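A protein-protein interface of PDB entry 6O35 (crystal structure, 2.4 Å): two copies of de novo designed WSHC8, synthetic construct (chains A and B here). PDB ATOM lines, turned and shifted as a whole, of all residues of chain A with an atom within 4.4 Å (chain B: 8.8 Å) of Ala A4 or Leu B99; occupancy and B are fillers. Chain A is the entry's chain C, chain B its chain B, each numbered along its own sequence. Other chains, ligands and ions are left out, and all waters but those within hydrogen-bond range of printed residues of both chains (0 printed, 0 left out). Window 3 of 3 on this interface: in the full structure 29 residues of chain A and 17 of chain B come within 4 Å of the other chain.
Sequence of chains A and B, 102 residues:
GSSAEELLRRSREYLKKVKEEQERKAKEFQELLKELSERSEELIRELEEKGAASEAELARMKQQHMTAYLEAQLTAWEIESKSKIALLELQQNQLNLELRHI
Ala A4 touches Leu B99 (CB to CD2, 3.7 Å). Leu B95 touches Leu A7. Leu A8 touches Leu B99. CD2 of His A101 touches CD1 of Leu B99, at 3.8 Å.
Ser A2 touches none of the printed residues of chain B. No residue of chain B comes within 4 Å of Ser A3. Of chain B, only Leu B99 (3.7 Å) comes within 4 Å of Ala A4. Printed residues of chain B within 4 Å of Leu A7: Leu B95 (3.9 Å). Printed residues of chain B within 4 Å of Leu A8: Leu B99. Printed residues of chain B within 4 Å of His A101: Leu B99 (3.8 Å). Asn B93 touches none of the printed residues of chain A. Printed residues of chain A within 4 Å of Leu B95: Leu A7. Leu B99 touches just these residues of chain A: Ala A4, Leu A8 and His A101. The nearest printed residue of chain A that does not touch Leu B99 is Leu A7 (5.1 Å). The nearest printed residue of chain B that does not touch His A101 is Arg B100 (5.7 Å).
Of the 11 printed residues of chain B, 2 touch a printed residue of chain A. Hydrophobic or aromatic side chains of chain B within 4 Å of the printed part of chain A: Leu B95 and Leu B99. Among the printed residues, 4 pairs touch across the chains. Among the printed residues, no Asp or Glu carboxylate lies within 4 Å of a Lys or Arg side-chain nitrogen of the other chain.
Positions printed for both chains: 8 and 101.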
ATOM      1  N   SER A   2       7.371  34.705 -22.230  1.00  0.00           N
ATOM      2  CA  SER A   2       6.303  35.424 -22.983  1.00  0.00           C
ATOM      3  C   SER A   2       6.110  34.782 -24.354  1.00  0.00           C
ATOM      4  O   SER A   2       5.114  34.099 -24.594  1.00  0.00           O
ATOM      5  CB  SER A   2       6.649  36.903 -23.129  1.00  0.00           C
ATOM      6  N   SER A   3       7.071  35.011 -25.254  1.00  0.00           N
ATOM      7  CA  SER A   3       7.050  34.322 -26.540  1.00  0.00           C
ATOM      8  C   SER A   3       7.167  32.816 -26.348  1.00  0.00           C
ATOM      9  O   SER A   3       6.508  32.038 -27.047  1.00  0.00           O
ATOM     10  CB  SER A   3       8.177  34.841 -27.432  1.00  0.00           C
ATOM     11  N   ALA A   4       8.006  32.386 -25.401  1.00  0.00           N
ATOM     12  CA  ALA A   4       8.078  30.969 -25.065  1.00  0.00           C
ATOM     13  C   ALA A   4       6.763  30.486 -24.469  1.00  0.00           C
ATOM     14  O   ALA A   4       6.284  29.395 -24.801  1.00  0.00           O
ATOM     15  CB  ALA A   4       9.230  30.718 -24.093  1.00  0.00           C
ATOM     16  N   GLU A   5       6.165  31.284 -23.579  1.00  0.00           N
ATOM     17  CA  GLU A   5       4.868  30.928 -23.018  1.00  0.00           C
ATOM     18  C   GLU A   5       3.814  30.784 -24.106  1.00  0.00           C
ATOM     19  O   GLU A   5       2.885  29.980 -23.968  1.00  0.00           O
ATOM     20  CB  GLU A   5       4.436  31.979 -21.995  1.00  0.00           C
ATOM     21  N   GLU A   6       3.942  31.547 -25.195  1.00  0.00           N
ATOM     22  CA  GLU A   6       2.975  31.461 -26.283  1.00  0.00           C
ATOM     23  C   GLU A   6       3.164  30.183 -27.093  1.00  0.00           C
ATOM     24  O   GLU A   6       2.186  29.512 -27.438  1.00  0.00           O
ATOM     25  CB  GLU A   6       3.097  32.688 -27.187  1.00  0.00           C
ATOM     26  N   LEU A   7       4.413  29.835 -27.412  1.00  0.00           N
ATOM     27  CA  LEU A   7       4.668  28.613 -28.168  1.00  0.00           C
ATOM     28  C   LEU A   7       4.277  27.381 -27.362  1.00  0.00           C
ATOM     29  O   LEU A   7       3.587  26.489 -27.870  1.00  0.00           O
ATOM     30  CB  LEU A   7       6.139  28.546 -28.576  1.00  0.00           C
ATOM     31  CG  LEU A   7       6.508  29.364 -29.813  1.00  0.00           C
ATOM     32  N   LEU A   8       4.709  27.312 -26.102  1.00  0.00           N
ATOM     33  CA  LEU A   8       4.314  26.196 -25.250  1.00  0.00           C
ATOM     34  C   LEU A   8       2.799  26.123 -25.112  1.00  0.00           C
ATOM     35  O   LEU A   8       2.223  25.030 -25.073  1.00  0.00           O
ATOM     36  CB  LEU A   8       4.974  26.329 -23.880  1.00  0.00           C
ATOM     37  CG  LEU A   8       6.493  26.157 -23.868  1.00  0.00           C
ATOM     38  CD1 LEU A   8       7.070  26.596 -22.533  1.00  0.00           C
ATOM     39  CD2 LEU A   8       6.865  24.715 -24.173  1.00  0.00           C
ATOM     40  N   HIS A 101      10.926  25.981 -18.644  1.00  0.00           N
ATOM     41  CA  HIS A 101      10.918  27.252 -19.355  1.00  0.00           C
ATOM     42  C   HIS A 101       9.672  28.073 -19.044  1.00  0.00           C
ATOM     43  O   HIS A 101       9.183  28.822 -19.888  1.00  0.00           O
ATOM     44  CB  HIS A 101      11.014  27.006 -20.863  1.00  0.00           C
ATOM     45  CG  HIS A 101      11.710  28.100 -21.608  1.00  0.00           C
ATOM     46  ND1 HIS A 101      11.706  29.408 -21.179  1.00  0.00           N
ATOM     47  CD2 HIS A 101      12.445  28.076 -22.745  1.00  0.00           C
ATOM     48  CE1 HIS A 101      12.407  30.147 -22.022  1.00  0.00           C
ATOM     49  NE2 HIS A 101      12.862  29.363 -22.983  1.00  0.00           N
ATOM     50  N   LEU B   8      16.130  26.341 -38.523  1.00  0.00           N
ATOM     51  CA  LEU B   8      15.006  25.913 -37.698  1.00  0.00           C
ATOM     52  C   LEU B   8      13.670  26.283 -38.330  1.00  0.00           C
ATOM     53  O   LEU B   8      12.695  25.537 -38.190  1.00  0.00           O
ATOM     54  CB  LEU B   8      15.129  26.519 -36.302  1.00  0.00           C
ATOM     55  CG  LEU B   8      16.288  25.944 -35.484  1.00  0.00           C
ATOM     56  CD1 LEU B   8      16.686  26.882 -34.360  1.00  0.00           C
ATOM     57  CD2 LEU B   8      15.917  24.573 -34.932  1.00  0.00           C
ATOM     58  N   GLN B  92       7.887  18.141 -31.068  1.00  0.00           N
ATOM     59  CA  GLN B  92       8.353  18.554 -29.749  1.00  0.00           C
ATOM     60  C   GLN B  92       9.862  18.750 -29.740  1.00  0.00           C
ATOM     61  O   GLN B  92      10.365  19.713 -29.146  1.00  0.00           O
ATOM     62  CB  GLN B  92       7.933  17.530 -28.697  1.00  0.00           C
ATOM     63  CG  GLN B  92       6.616  17.859 -28.010  1.00  0.00           C
ATOM     64  CD  GLN B  92       6.201  16.808 -26.999  1.00  0.00           C
ATOM     65  OE1 GLN B  92       6.842  15.764 -26.875  1.00  0.00           O
ATOM     66  NE2 GLN B  92       5.123  17.079 -26.270  1.00  0.00           N
ATOM     67  N   ASN B  93      10.606  17.851 -30.390  1.00  0.00           N
ATOM     68  CA  ASN B  93      12.042  18.054 -30.544  1.00  0.00           C
ATOM     69  C   ASN B  93      12.324  19.382 -31.236  1.00  0.00           C
ATOM     70  O   ASN B  93      13.178  20.158 -30.797  1.00  0.00           O
ATOM     71  CB  ASN B  93      12.655  16.894 -31.329  1.00  0.00           C
ATOM     72  CG  ASN B  93      12.559  15.576 -30.590  1.00  0.00           C
ATOM     73  OD1 ASN B  93      12.791  15.510 -29.383  1.00  0.00           O
ATOM     74  ND2 ASN B  93      12.211  14.520 -31.312  1.00  0.00           N
ATOM     75  N   GLN B  94      11.610  19.655 -32.331  1.00  0.00           N
ATOM     76  CA  GLN B  94      11.743  20.941 -33.009  1.00  0.00           C
ATOM     77  C   GLN B  94      11.486  22.092 -32.045  1.00  0.00           C
ATOM     78  O   GLN B  94      12.311  23.003 -31.912  1.00  0.00           O
ATOM     79  CB  GLN B  94      10.775  20.994 -34.195  1.00  0.00           C
ATOM     80  CG  GLN B  94      10.747  22.313 -34.947  1.00  0.00           C
ATOM     81  CD  GLN B  94      11.985  22.538 -35.787  1.00  0.00           C
ATOM     82  OE1 GLN B  94      12.766  21.617 -36.027  1.00  0.00           O
ATOM     83  NE2 GLN B  94      12.174  23.771 -36.241  1.00  0.00           N
ATOM     84  N   LEU B  95      10.343  22.061 -31.358  1.00  0.00           N
ATOM     85  CA  LEU B  95      10.002  23.121 -30.412  1.00  0.00           C
ATOM     86  C   LEU B  95      11.101  23.303 -29.372  1.00  0.00           C
ATOM     87  O   LEU B  95      11.493  24.431 -29.057  1.00  0.00           O
ATOM     88  CB  LEU B  95       8.668  22.797 -29.743  1.00  0.00           C
ATOM     89  CG  LEU B  95       8.215  23.628 -28.543  1.00  0.00           C
ATOM     90  CD1 LEU B  95       7.650  24.968 -28.968  1.00  0.00           C
ATOM     91  CD2 LEU B  95       7.186  22.835 -27.738  1.00  0.00           C
ATOM     92  N   ASN B  96      11.604  22.197 -28.817  1.00  0.00           N
ATOM     93  CA  ASN B  96      12.679  22.292 -27.836  1.00  0.00           C
ATOM     94  C   ASN B  96      13.888  23.017 -28.415  1.00  0.00           C
ATOM     95  O   ASN B  96      14.528  23.820 -27.725  1.00  0.00           O
ATOM     96  CB  ASN B  96      13.078  20.897 -27.358  1.00  0.00           C
ATOM     97  CG  ASN B  96      14.297  20.917 -26.460  1.00  0.00           C
ATOM     98  OD1 ASN B  96      14.426  21.774 -25.584  1.00  0.00           O
ATOM     99  ND2 ASN B  96      15.207  19.975 -26.680  1.00  0.00           N
ATOM    100  N   LEU B  97      14.218  22.747 -29.679  1.00  0.00           N
ATOM    101  CA  LEU B  97      15.330  23.446 -30.311  1.00  0.00           C
ATOM    102  C   LEU B  97      15.032  24.937 -30.434  1.00  0.00           C
ATOM    103  O   LEU B  97      15.879  25.779 -30.117  1.00  0.00           O
ATOM    104  CB  LEU B  97      15.625  22.840 -31.682  1.00  0.00           C
ATOM    105  CG  LEU B  97      16.114  21.391 -31.712  1.00  0.00           C
ATOM    106  CD1 LEU B  97      16.604  21.030 -33.111  1.00  0.00           C
ATOM    107  CD2 LEU B  97      17.208  21.149 -30.685  1.00  0.00           C
ATOM    108  N   GLU B  98      13.823  25.280 -30.892  1.00  0.00           N
ATOM    109  CA  GLU B  98      13.442  26.686 -30.994  1.00  0.00           C
ATOM    110  C   GLU B  98      13.597  27.384 -29.649  1.00  0.00           C
ATOM    111  O   GLU B  98      14.212  28.453 -29.556  1.00  0.00           O
ATOM    112  CB  GLU B  98      12.006  26.807 -31.505  1.00  0.00           C
ATOM    113  CG  GLU B  98      11.727  26.009 -32.771  1.00  0.00           C
ATOM    114  CD  GLU B  98      10.596  26.587 -33.603  1.00  0.00           C
ATOM    115  OE1 GLU B  98       9.757  27.329 -33.048  1.00  0.00           O
ATOM    116  OE2 GLU B  98      10.554  26.305 -34.820  1.00  0.00           O
ATOM    117  N   LEU B  99      13.041  26.789 -28.590  1.00  0.00           N
ATOM    118  CA  LEU B  99      13.258  27.312 -27.247  1.00  0.00           C
ATOM    119  C   LEU B  99      14.747  27.392 -26.935  1.00  0.00           C
ATOM    120  O   LEU B  99      15.233  28.401 -26.409  1.00  0.00           O
ATOM    121  CB  LEU B  99      12.552  26.436 -26.215  1.00  0.00           C
ATOM    122  CG  LEU B  99      11.027  26.461 -26.144  1.00  0.00           C
ATOM    123  CD1 LEU B  99      10.558  25.645 -24.939  1.00  0.00           C
ATOM    124  CD2 LEU B  99      10.490  27.877 -26.072  1.00  0.00           C
ATOM    125  N   ARG B 100      15.490  26.326 -27.251  1.00  0.00           N
ATOM    126  CA  ARG B 100      16.920  26.303 -26.966  1.00  0.00           C
ATOM    127  C   ARG B 100      17.620  27.517 -27.558  1.00  0.00           C
ATOM    128  O   ARG B 100      18.556  28.057 -26.958  1.00  0.00           O
ATOM    129  CB  ARG B 100      17.539  25.013 -27.505  1.00  0.00           C
ATOM    130  N   HIS B 101      17.182  27.961 -28.732  1.00  0.00           N
ATOM    131  CA  HIS B 101      17.743  29.152 -29.359  1.00  0.00           C
ATOM    132  C   HIS B 101      16.919  30.386 -29.003  1.00  0.00           C
ATOM    133  O   HIS B 101      16.765  30.726 -27.831  1.00  0.00           O
ATOM    134  CB  HIS B 101      17.806  28.984 -30.877  1.00  0.00           C
ATOM    135  CG  HIS B 101      18.794  27.955 -31.331  1.00  0.00           C
ATOM    136  ND1 HIS B 101      18.870  26.698 -30.772  1.00  0.00           N
ATOM    137  CD2 HIS B 101      19.746  27.998 -32.292  1.00  0.00           C
ATOM    138  CE1 HIS B 101      19.827  26.010 -31.370  1.00  0.00           C
ATOM    139  NE2 HIS B 101      20.374  26.777 -32.296  1.00  0.00           N
